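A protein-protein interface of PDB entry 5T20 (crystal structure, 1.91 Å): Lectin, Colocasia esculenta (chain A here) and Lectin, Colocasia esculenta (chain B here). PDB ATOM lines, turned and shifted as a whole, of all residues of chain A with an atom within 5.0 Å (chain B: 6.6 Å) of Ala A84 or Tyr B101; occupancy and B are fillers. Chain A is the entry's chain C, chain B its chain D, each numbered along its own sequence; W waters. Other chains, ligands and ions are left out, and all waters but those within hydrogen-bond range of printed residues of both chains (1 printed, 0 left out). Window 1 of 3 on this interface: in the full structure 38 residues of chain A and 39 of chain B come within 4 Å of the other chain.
N of Val A100 is in hydrogen-bond range of O of Ile B100 (2.9 Å). N of Gly A97 sits at hydrogen-bond distance from O of Pro B103, at 3.0 Å. The backbone carbonyl oxygen (O) of Gly B102 lies close to the backbone carbonyl oxygen (O) of Gly A97. O of Pro A98 lies within hydrogen-bond range of N of Gly B102.
The backbone NH of Phe A96 lies within hydrogen-bond range of the backbone carbonyl oxygen of Ala A84, 2.8 Å away. The backbone NH (N) of Ile B91 sits at hydrogen-bond distance from the backbone carbonyl oxygen (O) of Val B99. The backbone NH (N) of Ser A99 is in hydrogen-bond range of the backbone carbonyl oxygen (O) of Asn A82 (3.0 Å). The backbone NH (N) of Val A86 sits at hydrogen-bond distance from the backbone carbonyl oxygen (O) of Val A94, at 2.7 Å. OH of Tyr B101 is in hydrogen-bond range of NH1 of Arg B93. The backbone carbonyl oxygen (O) of Asp B87 lies within hydrogen-bond range of the backbone NH (N) of Ala B104 (2.9 Å).
Leu A7 touches Tyr B101 (CD2 to OH, 3.5 Å). Ile B91 touches Ala A84. Ala A84 touches Tyr B101 (CB to CD2, 3.7 Å). Phe A96 touches Asp B87 (CD1 to O, 3.2 Å). CD2 of Phe A96 touches CG1 of Val B89, at 3.6 Å. Phe A96 touches Gly B102. O of Pro A98 touches CA of Tyr B101 (3.9 Å). Ser A99 touches Val B99. CB of Ser A99 touches CE1 of Tyr B101, at 3.9 Å. Val A100 touches Gly B64 (CG2 to O, 3.8 Å).
Of the printed residues of chain B, Ala A84 touches Ile B91 (3.7 Å) and Tyr B101 (3.7 Å). Printed residues of chain B within 4 Å of Val A94: Ala B104. Of the printed residues of chain A, Val B89 touches Phe A96. Tyr B101 touches just these residues of chain A: Leu A7 (3.5 Å), Asn A82 (3.4 Å), Tyr A83 (3.8 Å), Ala A84 (3.7 Å), Phe A96 (3.7 Å), Pro A98 (3.9 Å) and Ser A99 (3.9 Å). The nearest residue of chain A that does not touch Tyr B101 is Gly A97 (4.2 Å).
Of the 15 printed residues of chain A, 12 touch a printed residue of chain B. Among the printed residues, no Asp or Glu carboxylate lies within 4 Å of a Lys or Arg side-chain nitrogen of the other chain.
Water W1 lies within hydrogen-bond range of the side-chain hydroxyl (OH) of Tyr B101 and the backbone carbonyl oxygen (O) of Tyr A83.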
ATOM      1  N   LEU A   6     -19.811  -2.205   0.199  1.00  0.00           N
ATOM      2  CA  LEU A   6     -20.684  -1.220  -0.397  1.00  0.00           C
ATOM      3  C   LEU A   6     -20.443  -1.252  -1.900  1.00  0.00           C
ATOM      4  O   LEU A   6     -19.292  -1.161  -2.328  1.00  0.00           O
ATOM      5  CB  LEU A   6     -20.401   0.176   0.219  1.00  0.00           C
ATOM      6  CG  LEU A   6     -21.214   1.356  -0.317  1.00  0.00           C
ATOM      7  CD1 LEU A   6     -22.690   1.250   0.076  1.00  0.00           C
ATOM      8  CD2 LEU A   6     -20.626   2.647   0.161  1.00  0.00           C
ATOM      9  N   LEU A   7     -21.521  -1.388  -2.694  1.00  0.00           N
ATOM     10  CA  LEU A   7     -21.443  -1.437  -4.153  1.00  0.00           C
ATOM     11  C   LEU A   7     -21.725  -0.092  -4.764  1.00  0.00           C
ATOM     12  O   LEU A   7     -22.400   0.724  -4.147  1.00  0.00           O
ATOM     13  CB  LEU A   7     -22.425  -2.466  -4.727  1.00  0.00           C
ATOM     14  CG  LEU A   7     -22.309  -3.910  -4.197  1.00  0.00           C
ATOM     15  CD1 LEU A   7     -23.358  -4.794  -4.878  1.00  0.00           C
ATOM     16  CD2 LEU A   7     -20.903  -4.459  -4.383  1.00  0.00           C
ATOM     17  N   LEU A  55     -20.615   5.399  -3.520  1.00  0.00           N
ATOM     18  CA  LEU A  55     -19.505   4.878  -4.311  1.00  0.00           C
ATOM     19  C   LEU A  55     -19.886   5.088  -5.761  1.00  0.00           C
ATOM     20  O   LEU A  55     -20.932   4.608  -6.184  1.00  0.00           O
ATOM     21  CB  LEU A  55     -19.210   3.378  -3.962  1.00  0.00           C
ATOM     22  CG  LEU A  55     -18.055   2.691  -4.761  1.00  0.00           C
ATOM     23  CD1 LEU A  55     -16.690   3.325  -4.436  1.00  0.00           C
ATOM     24  CD2 LEU A  55     -17.967   1.194  -4.424  1.00  0.00           C
ATOM     25  N   ASN A  82     -18.785  -1.141 -12.395  1.00  0.00           N
ATOM     26  CA  ASN A  82     -19.313  -1.560 -11.093  1.00  0.00           C
ATOM     27  C   ASN A  82     -18.168  -1.794 -10.109  1.00  0.00           C
ATOM     28  O   ASN A  82     -17.316  -2.656 -10.326  1.00  0.00           O
ATOM     29  CB  ASN A  82     -20.134  -2.842 -11.239  1.00  0.00           C
ATOM     30  CG  ASN A  82     -21.192  -2.794 -12.296  1.00  0.00           C
ATOM     31  OD1 ASN A  82     -22.093  -1.978 -12.244  1.00  0.00           O
ATOM     32  ND2 ASN A  82     -21.125  -3.703 -13.249  1.00  0.00           N
ATOM     33  N   TYR A  83     -18.171  -1.053  -9.005  1.00  0.00           N
ATOM     34  CA  TYR A  83     -17.101  -1.140  -8.017  1.00  0.00           C
ATOM     35  C   TYR A  83     -17.616  -1.713  -6.717  1.00  0.00           C
ATOM     36  O   TYR A  83     -18.817  -1.739  -6.494  1.00  0.00           O
ATOM     37  CB  TYR A  83     -16.499   0.268  -7.779  1.00  0.00           C
ATOM     38  CG  TYR A  83     -15.638   0.726  -8.937  1.00  0.00           C
ATOM     39  CD1 TYR A  83     -14.248   0.626  -8.878  1.00  0.00           C
ATOM     40  CD2 TYR A  83     -16.211   1.107 -10.148  1.00  0.00           C
ATOM     41  CE1 TYR A  83     -13.454   0.966  -9.969  1.00  0.00           C
ATOM     42  CE2 TYR A  83     -15.424   1.424 -11.255  1.00  0.00           C
ATOM     43  CZ  TYR A  83     -14.048   1.339 -11.164  1.00  0.00           C
ATOM     44  OH  TYR A  83     -13.280   1.667 -12.257  1.00  0.00           O
ATOM     45  N   ALA A  84     -16.697  -2.089  -5.833  1.00  0.00           N
ATOM     46  CA  ALA A  84     -17.046  -2.574  -4.488  1.00  0.00           C
ATOM     47  C   ALA A  84     -16.047  -2.065  -3.469  1.00  0.00           C
ATOM     48  O   ALA A  84     -14.860  -2.248  -3.646  1.00  0.00           O
ATOM     49  CB  ALA A  84     -17.089  -4.102  -4.469  1.00  0.00           C
ATOM     50  N   ALA A  85     -16.532  -1.399  -2.415  1.00  0.00           N
ATOM     51  CA  ALA A  85     -15.704  -0.944  -1.297  1.00  0.00           C
ATOM     52  C   ALA A  85     -15.871  -2.012  -0.217  1.00  0.00           C
ATOM     53  O   ALA A  85     -16.991  -2.265   0.234  1.00  0.00           O
ATOM     54  CB  ALA A  85     -16.141   0.441  -0.815  1.00  0.00           C
ATOM     55  N   VAL A  86     -14.782  -2.695   0.125  1.00  0.00           N
ATOM     56  CA  VAL A  86     -14.799  -3.839   1.046  1.00  0.00           C
ATOM     57  C   VAL A  86     -13.986  -3.547   2.313  1.00  0.00           C
ATOM     58  O   VAL A  86     -12.858  -3.066   2.233  1.00  0.00           O
ATOM     59  CB  VAL A  86     -14.273  -5.116   0.331  1.00  0.00           C
ATOM     60  CG1 VAL A  86     -14.277  -6.336   1.261  1.00  0.00           C
ATOM     61  CG2 VAL A  86     -15.075  -5.408  -0.942  1.00  0.00           C
ATOM     62  N   VAL A  94     -11.153  -0.973   1.351  1.00  0.00           N
ATOM     63  CA  VAL A  94     -10.521  -1.041   0.026  1.00  0.00           C
ATOM     64  C   VAL A  94     -11.554  -0.975  -1.086  1.00  0.00           C
ATOM     65  O   VAL A  94     -12.522  -1.730  -1.072  1.00  0.00           O
ATOM     66  CB  VAL A  94      -9.658  -2.333  -0.118  1.00  0.00           C
ATOM     67  CG1 VAL A  94      -8.893  -2.345  -1.447  1.00  0.00           C
ATOM     68  CG2 VAL A  94      -8.684  -2.502   1.066  1.00  0.00           C
ATOM     69  N   VAL A  95     -11.283  -0.147  -2.099  1.00  0.00           N
ATOM     70  CA  VAL A  95     -12.165  -0.056  -3.269  1.00  0.00           C
ATOM     71  C   VAL A  95     -11.578  -0.928  -4.354  1.00  0.00           C
ATOM     72  O   VAL A  95     -10.422  -0.758  -4.735  1.00  0.00           O
ATOM     73  CB  VAL A  95     -12.418   1.400  -3.773  1.00  0.00           C
ATOM     74  CG1 VAL A  95     -13.301   1.383  -5.030  1.00  0.00           C
ATOM     75  CG2 VAL A  95     -13.067   2.253  -2.686  1.00  0.00           C
ATOM     76  N   PHE A  96     -12.363  -1.864  -4.837  1.00  0.00           N
ATOM     77  CA  PHE A  96     -11.950  -2.788  -5.892  1.00  0.00           C
ATOM     78  C   PHE A  96     -12.824  -2.585  -7.089  1.00  0.00           C
ATOM     79  O   PHE A  96     -14.033  -2.445  -6.943  1.00  0.00           O
ATOM     80  CB  PHE A  96     -12.077  -4.251  -5.419  1.00  0.00           C
ATOM     81  CG  PHE A  96     -11.247  -4.724  -4.242  1.00  0.00           C
ATOM     82  CD1 PHE A  96     -10.069  -5.432  -4.442  1.00  0.00           C
ATOM     83  CD2 PHE A  96     -11.727  -4.602  -2.938  1.00  0.00           C
ATOM     84  CE1 PHE A  96      -9.351  -5.963  -3.355  1.00  0.00           C
ATOM     85  CE2 PHE A  96     -11.012  -5.131  -1.855  1.00  0.00           C
ATOM     86  CZ  PHE A  96      -9.830  -5.800  -2.068  1.00  0.00           C
ATOM     87  N   GLY A  97     -12.243  -2.600  -8.270  1.00  0.00           N
ATOM     88  CA  GLY A  97     -13.079  -2.479  -9.449  1.00  0.00           C
ATOM     89  C   GLY A  97     -12.334  -2.175 -10.723  1.00  0.00           C
ATOM     90  O   GLY A  97     -11.156  -1.806 -10.683  1.00  0.00           O
ATOM     91  N   PRO A  98     -13.022  -2.280 -11.871  1.00  0.00           N
ATOM     92  CA  PRO A  98     -14.435  -2.669 -12.037  1.00  0.00           C
ATOM     93  C   PRO A  98     -14.630  -4.185 -11.930  1.00  0.00           C
ATOM     94  O   PRO A  98     -13.653  -4.915 -11.759  1.00  0.00           O
ATOM     95  CB  PRO A  98     -14.764  -2.138 -13.439  1.00  0.00           C
ATOM     96  CG  PRO A  98     -13.453  -2.285 -14.203  1.00  0.00           C
ATOM     97  CD  PRO A  98     -12.372  -1.993 -13.175  1.00  0.00           C
ATOM     98  N   SER A  99     -15.892  -4.654 -12.007  1.00  0.00           N
ATOM     99  CA  SER A  99     -16.210  -6.086 -12.012  1.00  0.00           C
ATOM    100  C   SER A  99     -15.659  -6.697 -13.302  1.00  0.00           C
ATOM    101  O   SER A  99     -15.700  -6.042 -14.340  1.00  0.00           O
ATOM    102  CB  SER A  99     -17.719  -6.302 -11.906  1.00  0.00           C
ATOM    103  OG  SER A  99     -18.395  -5.702 -13.002  1.00  0.00           O
ATOM    104  N   VAL A 100     -15.078  -7.893 -13.228  1.00  0.00           N
ATOM    105  CA  VAL A 100     -14.502  -8.593 -14.372  1.00  0.00           C
ATOM    106  C   VAL A 100     -15.232  -9.918 -14.633  1.00  0.00           C
ATOM    107  O   VAL A 100     -15.066 -10.488 -15.701  1.00  0.00           O
ATOM    108  CB  VAL A 100     -12.957  -8.811 -14.239  1.00  0.00           C
ATOM    109  CG1 VAL A 100     -12.207  -7.476 -14.147  1.00  0.00           C
ATOM    110  CG2 VAL A 100     -12.603  -9.715 -13.060  1.00  0.00           C
ATOM    111  N   LEU B  60      -8.387 -17.531  -6.488  1.00  0.00           N
ATOM    112  CA  LEU B  60      -8.476 -16.278  -7.224  1.00  0.00           C
ATOM    113  C   LEU B  60      -7.063 -15.718  -7.297  1.00  0.00           C
ATOM    114  O   LEU B  60      -6.428 -15.548  -6.250  1.00  0.00           O
ATOM    115  CB  LEU B  60      -9.460 -15.298  -6.503  1.00  0.00           C
ATOM    116  CG  LEU B  60      -9.628 -13.879  -7.077  1.00  0.00           C
ATOM    117  CD1 LEU B  60     -10.272 -13.878  -8.475  1.00  0.00           C
ATOM    118  CD2 LEU B  60     -10.427 -13.022  -6.144  1.00  0.00           C
ATOM    119  N   GLY B  64      -7.324 -11.393 -11.480  1.00  0.00           N
ATOM    120  CA  GLY B  64      -8.772 -11.539 -11.436  1.00  0.00           C
ATOM    121  C   GLY B  64      -9.331 -12.785 -12.059  1.00  0.00           C
ATOM    122  O   GLY B  64     -10.522 -12.832 -12.386  1.00  0.00           O
ATOM    123  N   ASP B  87      -4.727  -6.442  -6.737  1.00  0.00           N
ATOM    124  CA  ASP B  87      -5.494  -7.222  -5.762  1.00  0.00           C
ATOM    125  C   ASP B  87      -6.983  -7.264  -6.136  1.00  0.00           C
ATOM    126  O   ASP B  87      -7.599  -6.242  -6.390  1.00  0.00           O
ATOM    127  CB  ASP B  87      -5.325  -6.651  -4.339  1.00  0.00           C
ATOM    128  CG  ASP B  87      -3.880  -6.660  -3.843  1.00  0.00           C
ATOM    129  OD1 ASP B  87      -3.173  -7.641  -4.111  1.00  0.00           O
ATOM    130  OD2 ASP B  87      -3.462  -5.670  -3.213  1.00  0.00           O
ATOM    131  N   TYR B  88      -7.551  -8.434  -6.115  1.00  0.00           N
ATOM    132  CA  TYR B  88      -8.957  -8.659  -6.442  1.00  0.00           C
ATOM    133  C   TYR B  88      -9.708  -9.275  -5.256  1.00  0.00           C
ATOM    134  O   TYR B  88      -9.087  -9.709  -4.281  1.00  0.00           O
ATOM    135  CB  TYR B  88      -9.050  -9.590  -7.672  1.00  0.00           C
ATOM    136  CG  TYR B  88      -8.624  -8.925  -8.968  1.00  0.00           C
ATOM    137  CD1 TYR B  88      -9.558  -8.586  -9.940  1.00  0.00           C
ATOM    138  CD2 TYR B  88      -7.286  -8.630  -9.218  1.00  0.00           C
ATOM    139  CE1 TYR B  88      -9.171  -7.980 -11.136  1.00  0.00           C
ATOM    140  CE2 TYR B  88      -6.896  -7.973 -10.382  1.00  0.00           C
ATOM    141  CZ  TYR B  88      -7.847  -7.632 -11.331  1.00  0.00           C
ATOM    142  OH  TYR B  88      -7.473  -7.035 -12.504  1.00  0.00           O
ATOM    143  N   VAL B  89     -11.049  -9.293  -5.346  1.00  0.00           N
ATOM    144  CA  VAL B  89     -11.892  -9.909  -4.346  1.00  0.00           C
ATOM    145  C   VAL B  89     -13.072 -10.556  -5.057  1.00  0.00           C
ATOM    146  O   VAL B  89     -13.590 -10.006  -6.022  1.00  0.00           O
ATOM    147  CB  VAL B  89     -12.334  -8.917  -3.220  1.00  0.00           C
ATOM    148  CG1 VAL B  89     -13.188  -7.763  -3.756  1.00  0.00           C
ATOM    149  CG2 VAL B  89     -13.050  -9.646  -2.076  1.00  0.00           C
ATOM    150  N   LEU B  90     -13.441 -11.744  -4.612  1.00  0.00           N
ATOM    151  CA  LEU B  90     -14.641 -12.424  -5.040  1.00  0.00           C
ATOM    152  C   LEU B  90     -15.660 -12.227  -3.916  1.00  0.00           C
ATOM    153  O   LEU B  90     -15.378 -12.581  -2.765  1.00  0.00           O
ATOM    154  CB  LEU B  90     -14.366 -13.913  -5.301  1.00  0.00           C
ATOM    155  CG  LEU B  90     -15.613 -14.824  -5.412  1.00  0.00           C
ATOM    156  CD1 LEU B  90     -16.408 -14.551  -6.713  1.00  0.00           C
ATOM    157  CD2 LEU B  90     -15.208 -16.312  -5.307  1.00  0.00           C
ATOM    158  N   ILE B  91     -16.829 -11.658  -4.232  1.00  0.00           N
ATOM    159  CA  ILE B  91     -17.849 -11.443  -3.226  1.00  0.00           C
ATOM    160  C   ILE B  91     -19.076 -12.282  -3.559  1.00  0.00           C
ATOM    161  O   ILE B  91     -19.632 -12.133  -4.641  1.00  0.00           O
ATOM    162  CB  ILE B  91     -18.257  -9.941  -3.073  1.00  0.00           C
ATOM    163  CG1 ILE B  91     -17.014  -8.989  -2.944  1.00  0.00           C
ATOM    164  CG2 ILE B  91     -19.257  -9.763  -1.896  1.00  0.00           C
ATOM    165  CD1 ILE B  91     -17.393  -7.471  -2.973  1.00  0.00           C
ATOM    166  N   ARG B  93     -22.408 -11.926  -3.012  1.00  0.00           N
ATOM    167  CA  ARG B  93     -23.261 -10.782  -2.596  1.00  0.00           C
ATOM    168  C   ARG B  93     -24.559 -11.218  -1.971  1.00  0.00           C
ATOM    169  O   ARG B  93     -25.027 -12.332  -2.235  1.00  0.00           O
ATOM    170  CB  ARG B  93     -23.526  -9.888  -3.840  1.00  0.00           C
ATOM    171  CG  ARG B  93     -22.190  -9.431  -4.438  1.00  0.00           C
ATOM    172  CD  ARG B  93     -22.278  -8.450  -5.586  1.00  0.00           C
ATOM    173  NE  ARG B  93     -23.490  -8.326  -6.227  1.00  0.00           N
ATOM    174  CZ  ARG B  93     -23.799  -7.524  -7.294  1.00  0.00           C
ATOM    175  NH1 ARG B  93     -22.869  -6.795  -7.882  1.00  0.00           N
ATOM    176  NH2 ARG B  93     -25.052  -7.463  -7.718  1.00  0.00           N
ATOM    177  N   VAL B  99     -19.435 -12.138  -7.594  1.00  0.00           N
ATOM    178  CA  VAL B  99     -18.806 -11.198  -8.526  1.00  0.00           C
ATOM    179  C   VAL B  99     -17.325 -10.984  -8.167  1.00  0.00           C
ATOM    180  O   VAL B  99     -16.978 -10.855  -6.997  1.00  0.00           O
ATOM    181  CB  VAL B  99     -19.575  -9.836  -8.555  1.00  0.00           C
ATOM    182  CG1 VAL B  99     -19.040  -8.896  -9.645  1.00  0.00           C
ATOM    183  CG2 VAL B  99     -21.097 -10.043  -8.750  1.00  0.00           C
ATOM    184  N   ILE B 100     -16.476 -10.918  -9.190  1.00  0.00           N
ATOM    185  CA  ILE B 100     -15.049 -10.632  -9.018  1.00  0.00           C
ATOM    186  C   ILE B 100     -14.816  -9.173  -9.324  1.00  0.00           C
ATOM    187  O   ILE B 100     -15.095  -8.730 -10.444  1.00  0.00           O
ATOM    188  CB  ILE B 100     -14.123 -11.528  -9.886  1.00  0.00           C
ATOM    189  CG1 ILE B 100     -14.367 -13.036  -9.624  1.00  0.00           C
ATOM    190  CG2 ILE B 100     -12.632 -11.144  -9.676  1.00  0.00           C
ATOM    191  CD1 ILE B 100     -13.604 -13.907 -10.508  1.00  0.00           C
ATOM    192  N   TYR B 101     -14.234  -8.439  -8.359  1.00  0.00           N
ATOM    193  CA  TYR B 101     -13.925  -7.013  -8.497  1.00  0.00           C
ATOM    194  C   TYR B 101     -12.439  -6.773  -8.357  1.00  0.00           C
ATOM    195  O   TYR B 101     -11.814  -7.309  -7.452  1.00  0.00           O
ATOM    196  CB  TYR B 101     -14.640  -6.180  -7.404  1.00  0.00           C
ATOM    197  CG  TYR B 101     -16.155  -6.166  -7.463  1.00  0.00           C
ATOM    198  CD1 TYR B 101     -16.832  -5.206  -8.203  1.00  0.00           C
ATOM    199  CD2 TYR B 101     -16.908  -7.031  -6.676  1.00  0.00           C
ATOM    200  CE1 TYR B 101     -18.227  -5.164  -8.234  1.00  0.00           C
ATOM    201  CE2 TYR B 101     -18.298  -6.984  -6.679  1.00  0.00           C
ATOM    202  CZ  TYR B 101     -18.955  -6.045  -7.456  1.00  0.00           C
ATOM    203  OH  TYR B 101     -20.321  -6.010  -7.482  1.00  0.00           O
ATOM    204  N   GLY B 102     -11.920  -5.865  -9.149  1.00  0.00           N
ATOM    205  CA  GLY B 102     -10.519  -5.500  -9.065  1.00  0.00           C
ATOM    206  C   GLY B 102     -10.005  -4.857 -10.326  1.00  0.00           C
ATOM    207  O   GLY B 102     -10.678  -4.873 -11.359  1.00  0.00           O
ATOM    208  N   PRO B 103      -8.752  -4.375 -10.289  1.00  0.00           N
ATOM    209  CA  PRO B 103      -7.847  -4.360  -9.121  1.00  0.00           C
ATOM    210  C   PRO B 103      -8.288  -3.359  -8.040  1.00  0.00           C
ATOM    211  O   PRO B 103      -9.227  -2.568  -8.238  1.00  0.00           O
ATOM    212  CB  PRO B 103      -6.508  -3.952  -9.750  1.00  0.00           C
ATOM    213  CG  PRO B 103      -6.893  -3.069 -10.892  1.00  0.00           C
ATOM    214  CD  PRO B 103      -8.131  -3.725 -11.461  1.00  0.00           C
ATOM    215  N   ALA B 104      -7.629  -3.428  -6.869  1.00  0.00           N
ATOM    216  CA  ALA B 104      -7.813  -2.473  -5.784  1.00  0.00           C
ATOM    217  C   ALA B 104      -7.279  -1.112  -6.272  1.00  0.00           C
ATOM    218  O   ALA B 104      -6.156  -1.061  -6.799  1.00  0.00           O
ATOM    219  CB  ALA B 104      -7.047  -2.941  -4.551  1.00  0.00           C
HETATM  220  O   HOH W   1     -20.861  -3.299  -7.881  1.00  0.00           O
